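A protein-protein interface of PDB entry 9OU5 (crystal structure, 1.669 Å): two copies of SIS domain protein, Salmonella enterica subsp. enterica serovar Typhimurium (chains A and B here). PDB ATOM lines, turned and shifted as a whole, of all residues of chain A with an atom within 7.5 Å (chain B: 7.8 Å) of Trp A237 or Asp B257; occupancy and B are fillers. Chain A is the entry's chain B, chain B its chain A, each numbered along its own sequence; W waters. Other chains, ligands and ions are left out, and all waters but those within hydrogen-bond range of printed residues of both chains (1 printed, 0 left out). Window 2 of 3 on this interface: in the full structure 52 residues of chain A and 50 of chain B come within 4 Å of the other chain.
Water W1 lies within hydrogen-bond range of the side-chain hydroxyl of Tyr B213 (2.6 Å), the backbone carbonyl oxygen of Trp A237 (2.7 Å), the side-chain hydroxyl of Thr B260 (2.8 Å) and the side-chain hydroxyl of Thr B256 (3.4 Å).
The backbone NH (N) of Ala B258 sits at hydrogen-bond distance from the side-chain hydroxyl (OG1) of Thr B256, at 3.0 Å.
The backbone carbonyl oxygen of Met A233 lies close to the side-chain amide oxygen of Gln A236.
Of chain B, only Thr B256, Asp B257 and Ala B258 come within 4 Å of Trp A237.
Asp B257 touches one residue of chain A.
Of the printed residues of chain B, Phe A232 touches Glu B254 (3.9 Å) and Thr B256 (3.6 Å).
Printed residues of chain A within 4 Å of Ile B238: Val A211 and Ile A238.
Printed residues of chain A within 4 Å of Tyr B213: Ile A238 (3.6 Å) and His A239 (3.0 Å).
Of the printed residues of chain A, Thr B256 touches Phe A232 (3.6 Å), Gln A236 (3.3 Å) and Trp A237 (2.8 Å).
Printed residues of chain B within 4 Å of Ile A238: Val B211 (3.9 Å), Tyr B213 (3.6 Å) and Ile B238 (3.8 Å).
The nearest residue of chain A that does not touch Asp B257 is Gln A236 (4.8 Å).
Among the printed residues, pairs that only touch across the chains: Val A211 with Ile B238, Phe A232 with Glu B254, Phe A232 with Thr B256, Gln A236 with Thr B256, Trp A237 with Asp B257, Trp A237 with Ala B258, Ile A238 with Val B211, Ile A238 with Tyr B213 and Ile A238 with Ile B238.
Of the 12 printed residues of chain B, 7 touch a printed residue of chain A.
Printed residues of chain B that touch a printed residue of chain A: Val B211, Tyr B213, Ile B238, Glu B254, Thr B256, Asp B257 and Ala B258.
Hydrophobic or aromatic side chains of chain B within 4 Å of the printed part of chain A: Val B211, Tyr B213, Ile B238 and Ala B258.
Along chain B the printed residues that touch a printed residue of chain A span positions 211 to 258.
Printed residues of chain A that touch a printed residue of chain B: Val A211, Phe A232, Gln A236, Trp A237, Ile A238 and His A239.
Hydrophobic or aromatic side chains of chain A within 4 Å of the printed part of chain B: Val A211, Phe A232, Trp A237, Ile A238 and His A239.
Among the printed residues, 12 pairs touch across the chains.
Among the printed residues, no Asp or Glu carboxylate lies within 4 Å of a Lys or Arg side-chain nitrogen of the other chain.
The side-chain carboxylate of Glu B254 sits at hydrogen-bond distance from a ring nitrogen (ND1) of His A239 (2.9 Å).
The side-chain hydroxyl (OH) of Tyr B213 is in hydrogen-bond range of the backbone NH (N) of His A239.
The backbone carbonyl oxygen of Trp A237 lies within hydrogen-bond range of the side-chain hydroxyl of Thr B256 (2.8 Å).
Val A211 touches Ile B238, and with the chains exchanged Ile A238 touches Val B211.
Ile A238 touches its own counterpart, Ile B238.
Of the 12 pairs that touch across the chains among the printed residues, 3 have their exchanged pair printed and touching as well.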
ATOM      1  N   ASP A 209      -8.473  35.176  24.712  1.00  0.00           N
ATOM      2  CA  ASP A 209      -8.358  33.833  24.177  1.00  0.00           C
ATOM      3  C   ASP A 209      -9.764  33.226  24.193  1.00  0.00           C
ATOM      4  O   ASP A 209     -10.609  33.689  24.954  1.00  0.00           O
ATOM      5  CB  ASP A 209      -7.215  33.121  24.879  1.00  0.00           C
ATOM      6  CG  ASP A 209      -5.842  33.621  24.459  1.00  0.00           C
ATOM      7  OD1 ASP A 209      -5.371  33.178  23.413  1.00  0.00           O
ATOM      8  OD2 ASP A 209      -5.261  34.477  25.155  1.00  0.00           O
ATOM      9  N   LYS A 210     -10.046  32.278  23.289  1.00  0.00           N
ATOM     10  CA  LYS A 210     -11.323  31.583  23.275  1.00  0.00           C
ATOM     11  C   LYS A 210     -11.125  30.109  23.638  1.00  0.00           C
ATOM     12  O   LYS A 210     -12.060  29.449  24.074  1.00  0.00           O
ATOM     13  CB  LYS A 210     -12.027  31.745  21.917  1.00  0.00           C
ATOM     14  N   VAL A 211      -9.913  29.598  23.442  1.00  0.00           N
ATOM     15  CA  VAL A 211      -9.589  28.207  23.717  1.00  0.00           C
ATOM     16  C   VAL A 211      -8.270  28.169  24.488  1.00  0.00           C
ATOM     17  O   VAL A 211      -7.321  28.879  24.139  1.00  0.00           O
ATOM     18  CB  VAL A 211      -9.493  27.447  22.375  1.00  0.00           C
ATOM     19  CG1 VAL A 211      -8.977  26.017  22.540  1.00  0.00           C
ATOM     20  CG2 VAL A 211     -10.828  27.441  21.631  1.00  0.00           C
ATOM     21  N   ILE A 231     -12.869  26.412  31.878  1.00  0.00           N
ATOM     22  CA  ILE A 231     -12.427  27.271  30.793  1.00  0.00           C
ATOM     23  C   ILE A 231     -13.497  27.349  29.703  1.00  0.00           C
ATOM     24  O   ILE A 231     -13.794  28.448  29.214  1.00  0.00           O
ATOM     25  CB  ILE A 231     -11.074  26.778  30.248  1.00  0.00           C
ATOM     26  CG1 ILE A 231      -9.940  27.092  31.220  1.00  0.00           C
ATOM     27  CG2 ILE A 231     -10.806  27.359  28.862  1.00  0.00           C
ATOM     28  CD1 ILE A 231      -8.655  26.310  30.964  1.00  0.00           C
ATOM     29  N   PHE A 232     -14.077  26.202  29.333  1.00  0.00           N
ATOM     30  CA  PHE A 232     -15.110  26.175  28.308  1.00  0.00           C
ATOM     31  C   PHE A 232     -16.367  26.929  28.791  1.00  0.00           C
ATOM     32  O   PHE A 232     -17.021  27.630  28.014  1.00  0.00           O
ATOM     33  CB  PHE A 232     -15.365  24.716  27.937  1.00  0.00           C
ATOM     34  CG  PHE A 232     -16.488  24.547  26.929  1.00  0.00           C
ATOM     35  CD1 PHE A 232     -16.386  25.100  25.655  1.00  0.00           C
ATOM     36  CD2 PHE A 232     -17.665  23.903  27.275  1.00  0.00           C
ATOM     37  CE1 PHE A 232     -17.411  24.950  24.730  1.00  0.00           C
ATOM     38  CE2 PHE A 232     -18.703  23.780  26.350  1.00  0.00           C
ATOM     39  CZ  PHE A 232     -18.583  24.321  25.087  1.00  0.00           C
ATOM     40  N   MET A 233     -16.714  26.808  30.080  1.00  0.00           N
ATOM     41  CA  MET A 233     -17.881  27.498  30.626  1.00  0.00           C
ATOM     42  C   MET A 233     -17.716  29.016  30.564  1.00  0.00           C
ATOM     43  O   MET A 233     -18.704  29.745  30.420  1.00  0.00           O
ATOM     44  CB  MET A 233     -18.153  27.093  32.071  1.00  0.00           C
ATOM     45  CG  MET A 233     -18.802  25.740  32.173  1.00  0.00           C
ATOM     46  SD  MET A 233     -18.766  25.103  33.858  1.00  0.00           S
ATOM     47  CE  MET A 233     -19.862  26.247  34.706  1.00  0.00           C
ATOM     48  N   GLU A 234     -16.471  29.483  30.670  1.00  0.00           N
ATOM     49  CA  GLU A 234     -16.138  30.896  30.645  1.00  0.00           C
ATOM     50  C   GLU A 234     -16.152  31.389  29.203  1.00  0.00           C
ATOM     51  O   GLU A 234     -16.872  32.338  28.900  1.00  0.00           O
ATOM     52  CB  GLU A 234     -14.789  31.178  31.300  1.00  0.00           C
ATOM     53  CG  GLU A 234     -14.367  32.646  31.285  1.00  0.00           C
ATOM     54  CD  GLU A 234     -15.439  33.598  31.813  1.00  0.00           C
ATOM     55  OE1 GLU A 234     -16.085  33.262  32.841  1.00  0.00           O
ATOM     56  OE2 GLU A 234     -15.639  34.685  31.207  1.00  0.00           O
ATOM     57  N   MET A 235     -15.375  30.726  28.336  1.00  0.00           N
ATOM     58  CA  MET A 235     -15.121  31.179  26.977  1.00  0.00           C
ATOM     59  C   MET A 235     -16.235  30.783  26.001  1.00  0.00           C
ATOM     60  O   MET A 235     -16.421  31.457  25.013  1.00  0.00           O
ATOM     61  CB  MET A 235     -13.814  30.591  26.424  1.00  0.00           C
ATOM     62  CG  MET A 235     -12.550  31.092  27.069  1.00  0.00           C
ATOM     63  SD  MET A 235     -12.629  32.882  27.268  1.00  0.00           S
ATOM     64  CE  MET A 235     -10.962  33.066  27.909  1.00  0.00           C
ATOM     65  N   GLN A 236     -16.872  29.629  26.203  1.00  0.00           N
ATOM     66  CA  GLN A 236     -18.043  29.193  25.458  1.00  0.00           C
ATOM     67  C   GLN A 236     -17.765  29.124  23.957  1.00  0.00           C
ATOM     68  O   GLN A 236     -18.621  29.490  23.164  1.00  0.00           O
ATOM     69  CB  GLN A 236     -19.243  30.081  25.807  1.00  0.00           C
ATOM     70  CG  GLN A 236     -19.776  29.807  27.213  1.00  0.00           C
ATOM     71  CD  GLN A 236     -20.689  30.889  27.747  1.00  0.00           C
ATOM     72  OE1 GLN A 236     -20.550  31.366  28.879  1.00  0.00           O
ATOM     73  NE2 GLN A 236     -21.634  31.294  26.917  1.00  0.00           N
ATOM     74  N   TRP A 237     -16.598  28.600  23.566  1.00  0.00           N
ATOM     75  CA  TRP A 237     -16.261  28.484  22.163  1.00  0.00           C
ATOM     76  C   TRP A 237     -16.109  27.010  21.760  1.00  0.00           C
ATOM     77  O   TRP A 237     -16.972  26.478  21.050  1.00  0.00           O
ATOM     78  CB  TRP A 237     -15.009  29.319  21.864  1.00  0.00           C
ATOM     79  CG  TRP A 237     -14.793  29.465  20.386  1.00  0.00           C
ATOM     80  CD1 TRP A 237     -13.786  28.935  19.631  1.00  0.00           C
ATOM     81  CD2 TRP A 237     -15.676  30.153  19.468  1.00  0.00           C
ATOM     82  NE1 TRP A 237     -13.973  29.256  18.311  1.00  0.00           N
ATOM     83  CE2 TRP A 237     -15.122  29.996  18.177  1.00  0.00           C
ATOM     84  CE3 TRP A 237     -16.870  30.875  19.608  1.00  0.00           C
ATOM     85  CZ2 TRP A 237     -15.724  30.536  17.038  1.00  0.00           C
ATOM     86  CZ3 TRP A 237     -17.470  31.403  18.479  1.00  0.00           C
ATOM     87  CH2 TRP A 237     -16.904  31.231  17.211  1.00  0.00           C
ATOM     88  N   ILE A 238     -14.997  26.380  22.186  1.00  0.00           N
ATOM     89  CA  ILE A 238     -14.700  24.982  21.889  1.00  0.00           C
ATOM     90  C   ILE A 238     -14.161  24.292  23.149  1.00  0.00           C
ATOM     91  O   ILE A 238     -13.269  24.814  23.815  1.00  0.00           O
ATOM     92  CB  ILE A 238     -13.688  24.875  20.745  1.00  0.00           C
ATOM     93  CG1 ILE A 238     -14.282  25.415  19.433  1.00  0.00           C
ATOM     94  CG2 ILE A 238     -13.185  23.433  20.573  1.00  0.00           C
ATOM     95  CD1 ILE A 238     -13.231  25.741  18.390  1.00  0.00           C
ATOM     96  N   HIS A 239     -14.716  23.118  23.459  1.00  0.00           N
ATOM     97  CA  HIS A 239     -14.200  22.273  24.521  1.00  0.00           C
ATOM     98  C   HIS A 239     -12.940  21.585  23.999  1.00  0.00           C
ATOM     99  O   HIS A 239     -13.015  20.684  23.173  1.00  0.00           O
ATOM    100  CB  HIS A 239     -15.275  21.282  24.972  1.00  0.00           C
ATOM    101  CG  HIS A 239     -14.859  20.410  26.098  1.00  0.00           C
ATOM    102  ND1 HIS A 239     -15.603  19.318  26.494  1.00  0.00           N
ATOM    103  CD2 HIS A 239     -13.801  20.472  26.925  1.00  0.00           C
ATOM    104  CE1 HIS A 239     -14.990  18.738  27.526  1.00  0.00           C
ATOM    105  NE2 HIS A 239     -13.901  19.430  27.815  1.00  0.00           N
ATOM    106  N   SER A 240     -11.788  22.034  24.471  1.00  0.00           N
ATOM    107  CA  SER A 240     -10.523  21.518  23.979  1.00  0.00           C
ATOM    108  C   SER A 240      -9.983  20.397  24.867  1.00  0.00           C
ATOM    109  O   SER A 240     -10.455  20.157  25.982  1.00  0.00           O
ATOM    110  CB  SER A 240      -9.495  22.636  23.847  1.00  0.00           C
ATOM    111  OG  SER A 240      -9.276  23.250  25.105  1.00  0.00           O
ATOM    112  N   VAL B 211     -12.790  22.185  13.192  1.00  0.00           N
ATOM    113  CA  VAL B 211     -12.985  21.456  14.438  1.00  0.00           C
ATOM    114  C   VAL B 211     -14.251  20.586  14.376  1.00  0.00           C
ATOM    115  O   VAL B 211     -15.346  21.049  14.029  1.00  0.00           O
ATOM    116  CB  VAL B 211     -13.020  22.407  15.647  1.00  0.00           C
ATOM    117  CG1 VAL B 211     -12.993  21.630  16.961  1.00  0.00           C
ATOM    118  CG2 VAL B 211     -11.846  23.378  15.615  1.00  0.00           C
ATOM    119  N   TYR B 213     -16.076  17.502  16.996  1.00  0.00           N
ATOM    120  CA  TYR B 213     -16.064  16.644  18.172  1.00  0.00           C
ATOM    121  C   TYR B 213     -16.293  15.196  17.746  1.00  0.00           C
ATOM    122  O   TYR B 213     -16.981  14.972  16.752  1.00  0.00           O
ATOM    123  CB  TYR B 213     -17.212  17.083  19.070  1.00  0.00           C
ATOM    124  CG  TYR B 213     -17.054  18.430  19.739  1.00  0.00           C
ATOM    125  CD1 TYR B 213     -15.956  18.727  20.540  1.00  0.00           C
ATOM    126  CD2 TYR B 213     -18.027  19.403  19.570  1.00  0.00           C
ATOM    127  CE1 TYR B 213     -15.840  19.954  21.171  1.00  0.00           C
ATOM    128  CE2 TYR B 213     -17.932  20.626  20.195  1.00  0.00           C
ATOM    129  CZ  TYR B 213     -16.828  20.906  20.990  1.00  0.00           C
ATOM    130  OH  TYR B 213     -16.776  22.110  21.601  1.00  0.00           O
ATOM    131  N   TRP B 237      -5.971  22.486  13.500  1.00  0.00           N
ATOM    132  CA  TRP B 237      -6.334  23.737  14.151  1.00  0.00           C
ATOM    133  C   TRP B 237      -6.308  23.557  15.670  1.00  0.00           C
ATOM    134  O   TRP B 237      -5.331  23.964  16.313  1.00  0.00           O
ATOM    135  CB  TRP B 237      -7.686  24.230  13.631  1.00  0.00           C
ATOM    136  CG  TRP B 237      -8.018  25.648  14.002  1.00  0.00           C
ATOM    137  CD1 TRP B 237      -9.126  26.078  14.669  1.00  0.00           C
ATOM    138  CD2 TRP B 237      -7.273  26.835  13.642  1.00  0.00           C
ATOM    139  NE1 TRP B 237      -9.092  27.438  14.805  1.00  0.00           N
ATOM    140  CE2 TRP B 237      -7.983  27.933  14.170  1.00  0.00           C
ATOM    141  CE3 TRP B 237      -6.087  27.071  12.931  1.00  0.00           C
ATOM    142  CZ2 TRP B 237      -7.540  29.248  14.014  1.00  0.00           C
ATOM    143  CZ3 TRP B 237      -5.660  28.372  12.751  1.00  0.00           C
ATOM    144  CH2 TRP B 237      -6.380  29.442  13.291  1.00  0.00           C
ATOM    145  N   ILE B 238      -7.355  22.902  16.214  1.00  0.00           N
ATOM    146  CA  ILE B 238      -7.548  22.703  17.647  1.00  0.00           C
ATOM    147  C   ILE B 238      -7.905  21.233  17.910  1.00  0.00           C
ATOM    148  O   ILE B 238      -8.786  20.678  17.248  1.00  0.00           O
ATOM    149  CB  ILE B 238      -8.656  23.614  18.200  1.00  0.00           C
ATOM    150  CG1 ILE B 238      -8.291  25.088  18.121  1.00  0.00           C
ATOM    151  CG2 ILE B 238      -9.043  23.218  19.629  1.00  0.00           C
ATOM    152  CD1 ILE B 238      -9.473  25.993  18.376  1.00  0.00           C
ATOM    153  N   GLU B 254     -21.705  20.866  24.551  1.00  0.00           N
ATOM    154  CA  GLU B 254     -20.735  21.442  23.625  1.00  0.00           C
ATOM    155  C   GLU B 254     -21.468  22.060  22.430  1.00  0.00           C
ATOM    156  O   GLU B 254     -21.227  21.695  21.279  1.00  0.00           O
ATOM    157  CB  GLU B 254     -19.721  20.369  23.200  1.00  0.00           C
ATOM    158  CG  GLU B 254     -18.728  19.956  24.292  1.00  0.00           C
ATOM    159  CD  GLU B 254     -19.239  18.996  25.357  1.00  0.00           C
ATOM    160  OE1 GLU B 254     -20.432  18.642  25.336  1.00  0.00           O
ATOM    161  OE2 GLU B 254     -18.433  18.576  26.203  1.00  0.00           O
ATOM    162  N   ILE B 255     -22.362  23.012  22.724  1.00  0.00           N
ATOM    163  CA  ILE B 255     -23.229  23.608  21.717  1.00  0.00           C
ATOM    164  C   ILE B 255     -23.094  25.124  21.824  1.00  0.00           C
ATOM    165  O   ILE B 255     -23.673  25.734  22.712  1.00  0.00           O
ATOM    166  CB  ILE B 255     -24.676  23.111  21.898  1.00  0.00           C
ATOM    167  CG1 ILE B 255     -24.765  21.592  21.623  1.00  0.00           C
ATOM    168  CG2 ILE B 255     -25.655  23.914  21.031  1.00  0.00           C
ATOM    169  CD1 ILE B 255     -26.097  20.959  21.970  1.00  0.00           C
ATOM    170  N   THR B 256     -22.285  25.710  20.934  1.00  0.00           N
ATOM    171  CA  THR B 256     -21.989  27.131  20.997  1.00  0.00           C
ATOM    172  C   THR B 256     -22.176  27.761  19.619  1.00  0.00           C
ATOM    173  O   THR B 256     -22.681  27.116  18.693  1.00  0.00           O
ATOM    174  CB  THR B 256     -20.565  27.323  21.529  1.00  0.00           C
ATOM    175  OG1 THR B 256     -19.646  26.987  20.487  1.00  0.00           O
ATOM    176  CG2 THR B 256     -20.316  26.518  22.794  1.00  0.00           C
ATOM    177  N   ASP B 257     -21.738  29.021  19.524  1.00  0.00           N
ATOM    178  CA  ASP B 257     -21.730  29.786  18.285  1.00  0.00           C
ATOM    179  C   ASP B 257     -20.553  29.382  17.409  1.00  0.00           C
ATOM    180  O   ASP B 257     -20.435  29.871  16.284  1.00  0.00           O
ATOM    181  CB  ASP B 257     -21.659  31.281  18.549  1.00  0.00           C
ATOM    182  CG  ASP B 257     -22.884  31.857  19.239  1.00  0.00           C
ATOM    183  OD1 ASP B 257     -24.006  31.453  18.865  1.00  0.00           O
ATOM    184  OD2 ASP B 257     -22.706  32.712  20.130  1.00  0.00           O
ATOM    185  N   ALA B 258     -19.678  28.507  17.929  1.00  0.00           N
ATOM    186  CA  ALA B 258     -18.736  27.836  17.057  1.00  0.00           C
ATOM    187  C   ALA B 258     -19.472  26.876  16.106  1.00  0.00           C
ATOM    188  O   ALA B 258     -18.912  26.509  15.079  1.00  0.00           O
ATOM    189  CB  ALA B 258     -17.691  27.134  17.891  1.00  0.00           C
ATOM    190  N   ASN B 259     -20.688  26.425  16.470  1.00  0.00           N
ATOM    191  CA  ASN B 259     -21.486  25.519  15.651  1.00  0.00           C
ATOM    192  C   ASN B 259     -20.673  24.279  15.253  1.00  0.00           C
ATOM    193  O   ASN B 259     -20.767  23.806  14.114  1.00  0.00           O
ATOM    194  CB  ASN B 259     -22.064  26.257  14.441  1.00  0.00           C
ATOM    195  CG  ASN B 259     -23.069  25.449  13.649  1.00  0.00           C
ATOM    196  OD1 ASN B 259     -23.406  25.845  12.528  1.00  0.00           O
ATOM    197  ND2 ASN B 259     -23.535  24.316  14.164  1.00  0.00           N
ATOM    198  N   THR B 260     -19.895  23.738  16.202  1.00  0.00           N
ATOM    199  CA  THR B 260     -19.015  22.597  15.946  1.00  0.00           C
ATOM    200  C   THR B 260     -19.847  21.344  15.616  1.00  0.00           C
ATOM    201  O   THR B 260     -20.788  20.964  16.326  1.00  0.00           O
ATOM    202  CB  THR B 260     -18.094  22.384  17.156  1.00  0.00           C
ATOM    203  OG1 THR B 260     -17.491  23.633  17.472  1.00  0.00           O
ATOM    204  CG2 THR B 260     -16.970  21.397  16.892  1.00  0.00           C
ATOM    205  N   ARG B 287     -28.230  19.595  15.504  1.00  0.00           N
ATOM    206  CA  ARG B 287     -26.803  19.808  15.334  1.00  0.00           C
ATOM    207  C   ARG B 287     -26.388  19.045  14.081  1.00  0.00           C
ATOM    208  O   ARG B 287     -27.083  18.131  13.642  1.00  0.00           O
ATOM    209  CB  ARG B 287     -26.033  19.469  16.615  1.00  0.00           C
ATOM    210  CG  ARG B 287     -26.437  20.346  17.794  1.00  0.00           C
ATOM    211  CD  ARG B 287     -25.550  21.571  18.076  1.00  0.00           C
ATOM    212  NE  ARG B 287     -25.719  22.796  17.282  1.00  0.00           N
ATOM    213  CZ  ARG B 287     -24.876  23.844  17.280  1.00  0.00           C
ATOM    214  NH1 ARG B 287     -23.751  23.829  17.976  1.00  0.00           N
ATOM    215  NH2 ARG B 287     -25.140  24.917  16.553  1.00  0.00           N
HETATM  216  O   HOH W   1     -17.879  24.069  20.219  1.00  0.00           O
